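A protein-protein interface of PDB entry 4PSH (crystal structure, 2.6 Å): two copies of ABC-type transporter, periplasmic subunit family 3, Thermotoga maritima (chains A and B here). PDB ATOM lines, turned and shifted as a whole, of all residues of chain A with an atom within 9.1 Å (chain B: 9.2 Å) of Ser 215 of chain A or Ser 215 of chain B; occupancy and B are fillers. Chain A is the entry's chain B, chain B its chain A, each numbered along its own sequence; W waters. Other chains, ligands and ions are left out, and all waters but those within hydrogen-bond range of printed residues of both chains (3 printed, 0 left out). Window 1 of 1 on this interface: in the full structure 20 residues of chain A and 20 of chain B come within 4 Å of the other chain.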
ATOM      1  N   LEU A 209     -19.311 -11.072 -21.900  1.00  0.00           N
ATOM      2  CA  LEU A 209     -19.418 -12.482 -21.645  1.00  0.00           C
ATOM      3  C   LEU A 209     -20.073 -12.759 -20.329  1.00  0.00           C
ATOM      4  O   LEU A 209     -21.059 -13.427 -20.239  1.00  0.00           O
ATOM      5  CB  LEU A 209     -18.033 -13.082 -21.603  1.00  0.00           C
ATOM      6  CG  LEU A 209     -17.289 -13.202 -22.914  1.00  0.00           C
ATOM      7  CD1 LEU A 209     -16.157 -14.145 -22.821  1.00  0.00           C
ATOM      8  CD2 LEU A 209     -18.209 -13.610 -23.973  1.00  0.00           C
ATOM      9  N   ARG A 210     -19.441 -12.269 -19.295  1.00  0.00           N
ATOM     10  CA  ARG A 210     -19.957 -12.210 -17.929  1.00  0.00           C
ATOM     11  C   ARG A 210     -21.455 -12.001 -17.846  1.00  0.00           C
ATOM     12  O   ARG A 210     -22.181 -12.616 -17.092  1.00  0.00           O
ATOM     13  CB  ARG A 210     -19.263 -11.046 -17.251  1.00  0.00           C
ATOM     14  CG  ARG A 210     -19.449 -10.929 -15.785  1.00  0.00           C
ATOM     15  CD  ARG A 210     -18.141 -10.612 -15.128  1.00  0.00           C
ATOM     16  NE  ARG A 210     -17.481  -9.465 -15.726  1.00  0.00           N
ATOM     17  CZ  ARG A 210     -16.193  -9.414 -16.009  1.00  0.00           C
ATOM     18  NH1 ARG A 210     -15.413 -10.446 -15.758  1.00  0.00           N
ATOM     19  NH2 ARG A 210     -15.691  -8.327 -16.542  1.00  0.00           N
ATOM     20  N   GLU A 211     -21.919 -11.086 -18.691  1.00  0.00           N
ATOM     21  CA  GLU A 211     -23.317 -10.674 -18.807  1.00  0.00           C
ATOM     22  C   GLU A 211     -24.261 -11.522 -19.693  1.00  0.00           C
ATOM     23  O   GLU A 211     -25.417 -11.655 -19.386  1.00  0.00           O
ATOM     24  CB  GLU A 211     -23.394  -9.199 -19.213  1.00  0.00           C
ATOM     25  CG  GLU A 211     -23.544  -8.218 -18.028  1.00  0.00           C
ATOM     26  CD  GLU A 211     -22.460  -7.152 -17.960  1.00  0.00           C
ATOM     27  OE1 GLU A 211     -21.515  -7.267 -17.138  1.00  0.00           O
ATOM     28  OE2 GLU A 211     -22.570  -6.184 -18.741  1.00  0.00           O
ATOM     29  N   LEU A 212     -23.777 -12.058 -20.801  1.00  0.00           N
ATOM     30  CA  LEU A 212     -24.436 -13.103 -21.559  1.00  0.00           C
ATOM     31  C   LEU A 212     -24.672 -14.380 -20.683  1.00  0.00           C
ATOM     32  O   LEU A 212     -25.606 -15.150 -20.960  1.00  0.00           O
ATOM     33  CB  LEU A 212     -23.671 -13.417 -22.838  1.00  0.00           C
ATOM     34  CG  LEU A 212     -23.796 -12.451 -24.022  1.00  0.00           C
ATOM     35  CD1 LEU A 212     -23.488 -13.194 -25.322  1.00  0.00           C
ATOM     36  CD2 LEU A 212     -25.183 -11.831 -24.113  1.00  0.00           C
ATOM     37  N   LYS A 213     -23.875 -14.560 -19.617  1.00  0.00           N
ATOM     38  CA  LYS A 213     -23.968 -15.727 -18.730  1.00  0.00           C
ATOM     39  C   LYS A 213     -24.880 -15.481 -17.515  1.00  0.00           C
ATOM     40  O   LYS A 213     -24.909 -16.271 -16.564  1.00  0.00           O
ATOM     41  CB  LYS A 213     -22.586 -16.213 -18.284  1.00  0.00           C
ATOM     42  CG  LYS A 213     -21.710 -16.670 -19.430  1.00  0.00           C
ATOM     43  CD  LYS A 213     -20.764 -17.736 -18.987  1.00  0.00           C
ATOM     44  CE  LYS A 213     -20.436 -18.631 -20.155  1.00  0.00           C
ATOM     45  NZ  LYS A 213     -19.420 -19.668 -19.796  1.00  0.00           N
ATOM     46  N   LYS A 214     -25.638 -14.389 -17.589  1.00  0.00           N
ATOM     47  CA  LYS A 214     -26.478 -13.900 -16.513  1.00  0.00           C
ATOM     48  C   LYS A 214     -27.986 -14.072 -16.854  1.00  0.00           C
ATOM     49  O   LYS A 214     -28.456 -13.573 -17.896  1.00  0.00           O
ATOM     50  CB  LYS A 214     -26.141 -12.414 -16.378  1.00  0.00           C
ATOM     51  CG  LYS A 214     -26.585 -11.746 -15.110  1.00  0.00           C
ATOM     52  CD  LYS A 214     -25.415 -11.603 -14.104  1.00  0.00           C
ATOM     53  CE  LYS A 214     -25.870 -10.790 -12.843  1.00  0.00           C
ATOM     54  NZ  LYS A 214     -26.518 -11.701 -11.811  1.00  0.00           N
ATOM     55  N   SER A 215     -28.755 -14.739 -15.991  1.00  0.00           N
ATOM     56  CA  SER A 215     -30.185 -15.018 -16.307  1.00  0.00           C
ATOM     57  C   SER A 215     -31.195 -13.953 -15.830  1.00  0.00           C
ATOM     58  O   SER A 215     -31.036 -13.398 -14.742  1.00  0.00           O
ATOM     59  CB  SER A 215     -30.613 -16.383 -15.762  1.00  0.00           C
ATOM     60  OG  SER A 215     -30.554 -16.404 -14.345  1.00  0.00           O
ATOM     61  N   PRO A 216     -32.249 -13.691 -16.627  1.00  0.00           N
ATOM     62  CA  PRO A 216     -33.254 -12.783 -16.054  1.00  0.00           C
ATOM     63  C   PRO A 216     -33.670 -13.198 -14.625  1.00  0.00           C
ATOM     64  O   PRO A 216     -33.907 -12.312 -13.757  1.00  0.00           O
ATOM     65  CB  PRO A 216     -34.431 -12.857 -17.046  1.00  0.00           C
ATOM     66  CG  PRO A 216     -33.781 -13.279 -18.389  1.00  0.00           C
ATOM     67  CD  PRO A 216     -32.564 -14.110 -18.022  1.00  0.00           C
ATOM     68  N   TYR A 217     -33.740 -14.501 -14.360  1.00  0.00           N
ATOM     69  CA  TYR A 217     -34.141 -14.941 -13.018  1.00  0.00           C
ATOM     70  C   TYR A 217     -33.182 -14.403 -11.950  1.00  0.00           C
ATOM     71  O   TYR A 217     -33.607 -13.889 -10.913  1.00  0.00           O
ATOM     72  CB  TYR A 217     -34.265 -16.473 -12.915  1.00  0.00           C
ATOM     73  CG  TYR A 217     -34.657 -16.994 -11.553  1.00  0.00           C
ATOM     74  CD1 TYR A 217     -33.677 -17.349 -10.604  1.00  0.00           C
ATOM     75  CD2 TYR A 217     -35.995 -17.124 -11.200  1.00  0.00           C
ATOM     76  CE1 TYR A 217     -34.015 -17.818  -9.342  1.00  0.00           C
ATOM     77  CE2 TYR A 217     -36.362 -17.608  -9.930  1.00  0.00           C
ATOM     78  CZ  TYR A 217     -35.366 -17.951  -9.010  1.00  0.00           C
ATOM     79  OH  TYR A 217     -35.729 -18.433  -7.765  1.00  0.00           O
ATOM     80  N   ASP A 218     -31.892 -14.515 -12.215  1.00  0.00           N
ATOM     81  CA  ASP A 218     -30.862 -14.041 -11.298  1.00  0.00           C
ATOM     82  C   ASP A 218     -30.893 -12.543 -11.123  1.00  0.00           C
ATOM     83  O   ASP A 218     -30.687 -12.056 -10.000  1.00  0.00           O
ATOM     84  CB  ASP A 218     -29.474 -14.490 -11.783  1.00  0.00           C
ATOM     85  CG  ASP A 218     -29.164 -15.922 -11.366  1.00  0.00           C
ATOM     86  OD1 ASP A 218     -29.860 -16.442 -10.477  1.00  0.00           O
ATOM     87  OD2 ASP A 218     -28.243 -16.532 -11.907  1.00  0.00           O
ATOM     88  N   VAL A 219     -31.141 -11.818 -12.217  1.00  0.00           N
ATOM     89  CA  VAL A 219     -31.319 -10.382 -12.144  1.00  0.00           C
ATOM     90  C   VAL A 219     -32.500 -10.065 -11.215  1.00  0.00           C
ATOM     91  O   VAL A 219     -32.359  -9.283 -10.242  1.00  0.00           O
ATOM     92  CB  VAL A 219     -31.475  -9.733 -13.554  1.00  0.00           C
ATOM     93  CG1 VAL A 219     -31.948  -8.284 -13.473  1.00  0.00           C
ATOM     94  CG2 VAL A 219     -30.178  -9.811 -14.271  1.00  0.00           C
ATOM     95  N   LEU A 220     -33.643 -10.693 -11.483  1.00  0.00           N
ATOM     96  CA  LEU A 220     -34.798 -10.531 -10.623  1.00  0.00           C
ATOM     97  C   LEU A 220     -34.501 -10.826  -9.151  1.00  0.00           C
ATOM     98  O   LEU A 220     -34.990 -10.105  -8.281  1.00  0.00           O
ATOM     99  CB  LEU A 220     -35.953 -11.374 -11.130  1.00  0.00           C
ATOM    100  CG  LEU A 220     -37.364 -11.147 -10.588  1.00  0.00           C
ATOM    101  CD1 LEU A 220     -37.854  -9.727 -10.788  1.00  0.00           C
ATOM    102  CD2 LEU A 220     -38.285 -12.128 -11.311  1.00  0.00           C
ATOM    103  N   ILE A 221     -33.705 -11.855  -8.860  1.00  0.00           N
ATOM    104  CA  ILE A 221     -33.369 -12.168  -7.463  1.00  0.00           C
ATOM    105  C   ILE A 221     -32.577 -10.994  -6.865  1.00  0.00           C
ATOM    106  O   ILE A 221     -32.929 -10.510  -5.774  1.00  0.00           O
ATOM    107  CB  ILE A 221     -32.577 -13.514  -7.286  1.00  0.00           C
ATOM    108  CG1 ILE A 221     -33.498 -14.727  -7.424  1.00  0.00           C
ATOM    109  CG2 ILE A 221     -31.751 -13.552  -5.942  1.00  0.00           C
ATOM    110  CD1 ILE A 221     -34.381 -14.998  -6.205  1.00  0.00           C
ATOM    111  N   GLU A 222     -31.541 -10.519  -7.578  1.00  0.00           N
ATOM    112  CA  GLU A 222     -30.767  -9.363  -7.101  1.00  0.00           C
ATOM    113  C   GLU A 222     -31.685  -8.174  -6.844  1.00  0.00           C
ATOM    114  O   GLU A 222     -31.474  -7.435  -5.861  1.00  0.00           O
ATOM    115  CB  GLU A 222     -29.704  -8.901  -8.093  1.00  0.00           C
ATOM    116  CG  GLU A 222     -28.436  -9.678  -8.113  1.00  0.00           C
ATOM    117  CD  GLU A 222     -27.675  -9.516  -9.477  1.00  0.00           C
ATOM    118  OE1 GLU A 222     -27.989  -8.569 -10.298  1.00  0.00           O
ATOM    119  OE2 GLU A 222     -26.762 -10.356  -9.721  1.00  0.00           O
ATOM    120  N   LYS A 223     -32.681  -7.981  -7.721  1.00  0.00           N
ATOM    121  CA  LYS A 223     -33.585  -6.843  -7.578  1.00  0.00           C
ATOM    122  C   LYS A 223     -34.366  -6.853  -6.257  1.00  0.00           C
ATOM    123  O   LYS A 223     -34.566  -5.812  -5.693  1.00  0.00           O
ATOM    124  CB  LYS A 223     -34.500  -6.693  -8.778  1.00  0.00           C
ATOM    125  CG  LYS A 223     -35.600  -5.687  -8.561  1.00  0.00           C
ATOM    126  CD  LYS A 223     -36.343  -5.390  -9.855  1.00  0.00           C
ATOM    127  CE  LYS A 223     -37.486  -4.500  -9.499  1.00  0.00           C
ATOM    128  NZ  LYS A 223     -38.502  -4.335 -10.598  1.00  0.00           N
ATOM    129  N   LEU B 209     -41.283 -19.723 -17.158  1.00  0.00           N
ATOM    130  CA  LEU B 209     -40.379 -19.997 -16.021  1.00  0.00           C
ATOM    131  C   LEU B 209     -38.974 -20.551 -16.403  1.00  0.00           C
ATOM    132  O   LEU B 209     -37.948 -20.121 -15.830  1.00  0.00           O
ATOM    133  CB  LEU B 209     -41.035 -20.893 -14.958  1.00  0.00           C
ATOM    134  CG  LEU B 209     -42.169 -20.329 -14.100  1.00  0.00           C
ATOM    135  CD1 LEU B 209     -42.674 -21.360 -13.070  1.00  0.00           C
ATOM    136  CD2 LEU B 209     -41.784 -19.016 -13.417  1.00  0.00           C
ATOM    137  N   ARG B 210     -38.924 -21.534 -17.318  1.00  0.00           N
ATOM    138  CA  ARG B 210     -37.629 -22.099 -17.740  1.00  0.00           C
ATOM    139  C   ARG B 210     -36.799 -21.109 -18.573  1.00  0.00           C
ATOM    140  O   ARG B 210     -35.562 -21.130 -18.471  1.00  0.00           O
ATOM    141  CB  ARG B 210     -37.816 -23.385 -18.504  1.00  0.00           C
ATOM    142  CG  ARG B 210     -38.401 -24.466 -17.654  1.00  0.00           C
ATOM    143  CD  ARG B 210     -39.011 -25.530 -18.490  1.00  0.00           C
ATOM    144  NE  ARG B 210     -39.834 -26.344 -17.614  1.00  0.00           N
ATOM    145  CZ  ARG B 210     -40.373 -27.507 -17.947  1.00  0.00           C
ATOM    146  NH1 ARG B 210     -40.146 -28.004 -19.147  1.00  0.00           N
ATOM    147  NH2 ARG B 210     -41.099 -28.169 -17.060  1.00  0.00           N
ATOM    148  N   GLU B 211     -37.465 -20.237 -19.354  1.00  0.00           N
ATOM    149  CA  GLU B 211     -36.738 -19.220 -20.131  1.00  0.00           C
ATOM    150  C   GLU B 211     -36.069 -18.210 -19.212  1.00  0.00           C
ATOM    151  O   GLU B 211     -34.926 -17.843 -19.444  1.00  0.00           O
ATOM    152  CB  GLU B 211     -37.627 -18.514 -21.146  1.00  0.00           C
ATOM    153  CG  GLU B 211     -38.133 -19.426 -22.250  1.00  0.00           C
ATOM    154  CD  GLU B 211     -36.984 -20.247 -22.901  1.00  0.00           C
ATOM    155  OE1 GLU B 211     -36.977 -21.508 -22.732  1.00  0.00           O
ATOM    156  OE2 GLU B 211     -36.076 -19.624 -23.555  1.00  0.00           O
ATOM    157  N   LEU B 212     -36.782 -17.787 -18.167  1.00  0.00           N
ATOM    158  CA  LEU B 212     -36.288 -16.859 -17.173  1.00  0.00           C
ATOM    159  C   LEU B 212     -34.998 -17.343 -16.554  1.00  0.00           C
ATOM    160  O   LEU B 212     -34.113 -16.525 -16.291  1.00  0.00           O
ATOM    161  CB  LEU B 212     -37.330 -16.630 -16.071  1.00  0.00           C
ATOM    162  CG  LEU B 212     -38.110 -15.331 -16.060  1.00  0.00           C
ATOM    163  CD1 LEU B 212     -37.957 -14.534 -17.364  1.00  0.00           C
ATOM    164  CD2 LEU B 212     -39.588 -15.546 -15.748  1.00  0.00           C
ATOM    165  N   LYS B 213     -34.883 -18.653 -16.329  1.00  0.00           N
ATOM    166  CA  LYS B 213     -33.689 -19.204 -15.727  1.00  0.00           C
ATOM    167  C   LYS B 213     -32.567 -19.510 -16.726  1.00  0.00           C
ATOM    168  O   LYS B 213     -31.559 -20.126 -16.369  1.00  0.00           O
ATOM    169  CB  LYS B 213     -34.022 -20.451 -14.901  1.00  0.00           C
ATOM    170  CG  LYS B 213     -34.796 -20.177 -13.621  1.00  0.00           C
ATOM    171  CD  LYS B 213     -35.055 -21.465 -12.866  1.00  0.00           C
ATOM    172  CE  LYS B 213     -35.333 -21.146 -11.377  1.00  0.00           C
ATOM    173  NZ  LYS B 213     -35.643 -22.359 -10.522  1.00  0.00           N
ATOM    174  N   LYS B 214     -32.749 -19.094 -17.977  1.00  0.00           N
ATOM    175  CA  LYS B 214     -31.780 -19.359 -19.058  1.00  0.00           C
ATOM    176  C   LYS B 214     -31.048 -18.055 -19.360  1.00  0.00           C
ATOM    177  O   LYS B 214     -31.706 -17.067 -19.758  1.00  0.00           O
ATOM    178  CB  LYS B 214     -32.516 -19.824 -20.336  1.00  0.00           C
ATOM    179  CG  LYS B 214     -32.598 -21.303 -20.529  1.00  0.00           C
ATOM    180  CD  LYS B 214     -33.738 -21.638 -21.484  1.00  0.00           C
ATOM    181  CE  LYS B 214     -34.239 -23.090 -21.328  1.00  0.00           C
ATOM    182  NZ  LYS B 214     -35.051 -23.476 -22.555  1.00  0.00           N
ATOM    183  N   SER B 215     -29.718 -18.022 -19.173  1.00  0.00           N
ATOM    184  CA  SER B 215     -28.932 -16.833 -19.587  1.00  0.00           C
ATOM    185  C   SER B 215     -28.973 -16.697 -21.116  1.00  0.00           C
ATOM    186  O   SER B 215     -29.392 -17.636 -21.790  1.00  0.00           O
ATOM    187  CB  SER B 215     -27.523 -16.887 -19.041  1.00  0.00           C
ATOM    188  OG  SER B 215     -26.832 -18.021 -19.496  1.00  0.00           O
ATOM    189  N   PRO B 216     -28.618 -15.531 -21.685  1.00  0.00           N
ATOM    190  CA  PRO B 216     -28.687 -15.612 -23.185  1.00  0.00           C
ATOM    191  C   PRO B 216     -27.629 -16.565 -23.750  1.00  0.00           C
ATOM    192  O   PRO B 216     -27.769 -17.033 -24.894  1.00  0.00           O
ATOM    193  CB  PRO B 216     -28.451 -14.158 -23.672  1.00  0.00           C
ATOM    194  CG  PRO B 216     -28.739 -13.281 -22.504  1.00  0.00           C
ATOM    195  CD  PRO B 216     -28.561 -14.132 -21.201  1.00  0.00           C
ATOM    196  N   TYR B 217     -26.612 -16.867 -22.940  1.00  0.00           N
ATOM    197  CA  TYR B 217     -25.664 -17.904 -23.275  1.00  0.00           C
ATOM    198  C   TYR B 217     -26.321 -19.290 -23.440  1.00  0.00           C
ATOM    199  O   TYR B 217     -26.095 -19.958 -24.477  1.00  0.00           O
ATOM    200  CB  TYR B 217     -24.598 -17.981 -22.225  1.00  0.00           C
ATOM    201  CG  TYR B 217     -23.604 -19.067 -22.471  1.00  0.00           C
ATOM    202  CD1 TYR B 217     -22.506 -18.841 -23.288  1.00  0.00           C
ATOM    203  CD2 TYR B 217     -23.723 -20.316 -21.851  1.00  0.00           C
ATOM    204  CE1 TYR B 217     -21.556 -19.831 -23.497  1.00  0.00           C
ATOM    205  CE2 TYR B 217     -22.773 -21.315 -22.048  1.00  0.00           C
ATOM    206  CZ  TYR B 217     -21.702 -21.062 -22.889  1.00  0.00           C
ATOM    207  OH  TYR B 217     -20.744 -22.005 -23.127  1.00  0.00           O
ATOM    208  N   ASP B 218     -27.115 -19.702 -22.427  1.00  0.00           N
ATOM    209  CA  ASP B 218     -27.811 -20.989 -22.404  1.00  0.00           C
ATOM    210  C   ASP B 218     -28.741 -21.088 -23.597  1.00  0.00           C
ATOM    211  O   ASP B 218     -28.824 -22.125 -24.266  1.00  0.00           O
ATOM    212  CB  ASP B 218     -28.632 -21.153 -21.116  1.00  0.00           C
ATOM    213  CG  ASP B 218     -27.782 -21.172 -19.833  1.00  0.00           C
ATOM    214  OD1 ASP B 218     -26.698 -21.783 -19.825  1.00  0.00           O
ATOM    215  OD2 ASP B 218     -28.216 -20.580 -18.805  1.00  0.00           O
ATOM    216  N   VAL B 219     -29.432 -19.996 -23.885  1.00  0.00           N
ATOM    217  CA  VAL B 219     -30.305 -19.941 -25.058  1.00  0.00           C
ATOM    218  C   VAL B 219     -29.482 -20.112 -26.334  1.00  0.00           C
ATOM    219  O   VAL B 219     -29.931 -20.729 -27.269  1.00  0.00           O
ATOM    220  CB  VAL B 219     -31.133 -18.579 -25.115  1.00  0.00           C
ATOM    221  CG1 VAL B 219     -31.816 -18.372 -26.438  1.00  0.00           C
ATOM    222  CG2 VAL B 219     -32.161 -18.517 -23.969  1.00  0.00           C
ATOM    223  N   LEU B 220     -28.277 -19.554 -26.383  1.00  0.00           N
ATOM    224  CA  LEU B 220     -27.457 -19.662 -27.604  1.00  0.00           C
ATOM    225  C   LEU B 220     -26.949 -21.091 -27.831  1.00  0.00           C
ATOM    226  O   LEU B 220     -26.981 -21.594 -28.962  1.00  0.00           O
ATOM    227  CB  LEU B 220     -26.301 -18.666 -27.578  1.00  0.00           C
ATOM    228  CG  LEU B 220     -25.445 -18.536 -28.837  1.00  0.00           C
ATOM    229  CD1 LEU B 220     -26.279 -18.180 -30.079  1.00  0.00           C
ATOM    230  CD2 LEU B 220     -24.395 -17.473 -28.545  1.00  0.00           C
ATOM    231  N   ILE B 221     -26.501 -21.726 -26.746  1.00  0.00           N
ATOM    232  CA  ILE B 221     -26.155 -23.136 -26.726  1.00  0.00           C
ATOM    233  C   ILE B 221     -27.296 -23.962 -27.261  1.00  0.00           C
ATOM    234  O   ILE B 221     -27.090 -24.741 -28.166  1.00  0.00           O
ATOM    235  CB  ILE B 221     -25.830 -23.610 -25.319  1.00  0.00           C
ATOM    236  CG1 ILE B 221     -24.580 -22.905 -24.829  1.00  0.00           C
ATOM    237  CG2 ILE B 221     -25.591 -25.110 -25.283  1.00  0.00           C
ATOM    238  CD1 ILE B 221     -23.328 -23.454 -25.430  1.00  0.00           C
ATOM    239  N   GLU B 222     -28.501 -23.774 -26.718  1.00  0.00           N
ATOM    240  CA  GLU B 222     -29.681 -24.470 -27.222  1.00  0.00           C
ATOM    241  C   GLU B 222     -29.899 -24.337 -28.761  1.00  0.00           C
ATOM    242  O   GLU B 222     -30.315 -25.328 -29.459  1.00  0.00           O
ATOM    243  CB  GLU B 222     -30.950 -24.084 -26.427  1.00  0.00           C
ATOM    244  CG  GLU B 222     -31.079 -24.911 -25.174  1.00  0.00           C
ATOM    245  CD  GLU B 222     -32.327 -24.625 -24.378  1.00  0.00           C
ATOM    246  OE1 GLU B 222     -33.204 -23.931 -24.919  1.00  0.00           O
ATOM    247  OE2 GLU B 222     -32.437 -25.091 -23.209  1.00  0.00           O
HETATM  248  O   HOH W   1     -18.353 -21.986 -20.700  1.00  0.00           O
HETATM  249  O   HOH W   2     -24.995 -19.234 -17.921  1.00  0.00           O
HETATM  250  O   HOH W   3     -30.885 -19.031 -13.445  1.00  0.00           O
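Water W1 bridges NZ of Lys 213 of chain A and OH of Tyr 217 of chain B.
Water W2 lies within hydrogen-bond range of the side-chain hydroxyl (OG) of Ser 215 of chain B (2.7 Å) and the backbone carbonyl oxygen (O) of Lys 213 of chain A (3.3 Å).
Water W3 bridges the side-chain hydroxyl of Ser 215 of chain A (2.8 Å) and the backbone carbonyl oxygen of Lys 213 of chain B (3.2 Å).
NZ of Lys 214 of chain B lies within salt-bridge range of OE1 of Glu 211 of chain B (2.8 Å).
OE1 of Glu 222 of chain B is in salt-bridge range of NZ of Lys 214 of chain B.
The backbone NH of Ser 215 of chain B sits at hydrogen-bond distance from the side-chain carboxylate of Asp 218 of chain B (3.0 Å).
The side-chain amino group of Lys 214 of chain A lies within salt-bridge range of the side-chain carboxylate of Glu 222 of chain A (2.5 Å).
The side-chain hydroxyl (OG) of Ser 215 of chain A is in hydrogen-bond range of the backbone NH (N) of Asp 218 of chain A, at 3.1 Å.
Among the printed residues, pairs that only touch across the chains: Lys 214 of chain A with Pro 216 of chain B, Lys 213 of chain A with Ser 215 of chain B, Lys 214 of chain A with Ser 215 of chain B, Pro 216 of chain A with Lys 214 of chain B, Ser 215 of chain A with Leu 212 of chain B, Lys 213 of chain A with Tyr 217 of chain B, Tyr 217 of chain A with Lys 213 of chain B, Ser 215 of chain A with Lys 213 of chain B, Ser 215 of chain A with Ser 215 of chain B and Ser 215 of chain A with Lys 214 of chain B.
Leu 212 of chain A touches Pro 216 of chain B, and with the chains exchanged Pro 216 of chain A touches Leu 212 of chain B.
Leu 212 of chain A touches Tyr 217 of chain B, and with the chains exchanged Tyr 217 of chain A touches Leu 212 of chain B.
Lys 214 of chain A touches Ser 215 of chain B, and with the chains exchanged Ser 215 of chain A touches Lys 214 of chain B.
Ser 215 of chain A touches its own counterpart, Ser 215 of chain B.
14 positions are printed for both chains.
Of the 15 pairs that touch across the chains among the printed residues, 15 have their exchanged pair printed and touching as well.
The backbone carbonyl oxygen (O) of Leu 212 of chain B lies within hydrogen-bond range of the backbone NH (N) of Tyr 217 of chain A, 2.8 Å away.
OG of Ser 215 of chain B sits close to O of Leu 212 of chain A (3.4 Å).
The backbone carbonyl oxygen (O) of Leu 212 of chain A sits at hydrogen-bond distance from the backbone NH (N) of Tyr 217 of chain B.
The backbone carbonyl oxygen of Leu 212 of chain A lies close to the backbone nitrogen of Pro 216 of chain B, 3.1 Å away.
N of Pro 216 of chain A lies close to O of Leu 212 of chain B, at 3.4 Å.
Printed residues of chain B within 4 Å of Ser 215 of chain A: Leu 212 (3.5 Å), Lys 213 (3.8 Å), Lys 214 (3.99 Å) and Ser 215 (3.9 Å).
Ser 215 of chain B touches just these residues of chain A: Leu 212, Lys 213, Lys 214 and Ser 215.
No residue of chain B comes within 4 Å of Asp 218 of chain A.
Pro 216 of chain B touches just these residues of chain A: Leu 212 (3.1 Å) and Lys 214 (3.4 Å).
Of the printed residues of chain A, Lys 213 of chain B touches Ser 215 and Tyr 217.
Of the printed residues of chain B, Leu 212 of chain A touches Ser 215, Pro 216 and Tyr 217.
Printed residues of chain A within 4 Å of Tyr 217 of chain B: Leu 212 and Lys 213.
Asp 218 of chain B touches none of the printed residues of chain A.
The nearest printed residue of chain B that does not touch Ser 215 of chain A is Pro 216 of chain B (5.2 Å).
The nearest printed residue of chain B that does not touch Tyr 217 of chain A is Leu 209 of chain B (5.9 Å).
Of the 15 printed residues of chain A, 6 touch a printed residue of chain B.
Of the 14 printed residues of chain B, 6 touch a printed residue of chain A.
Among the printed residues, no Asp or Glu carboxylate lies within 4 Å of a Lys or Arg side-chain nitrogen of the other chain.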
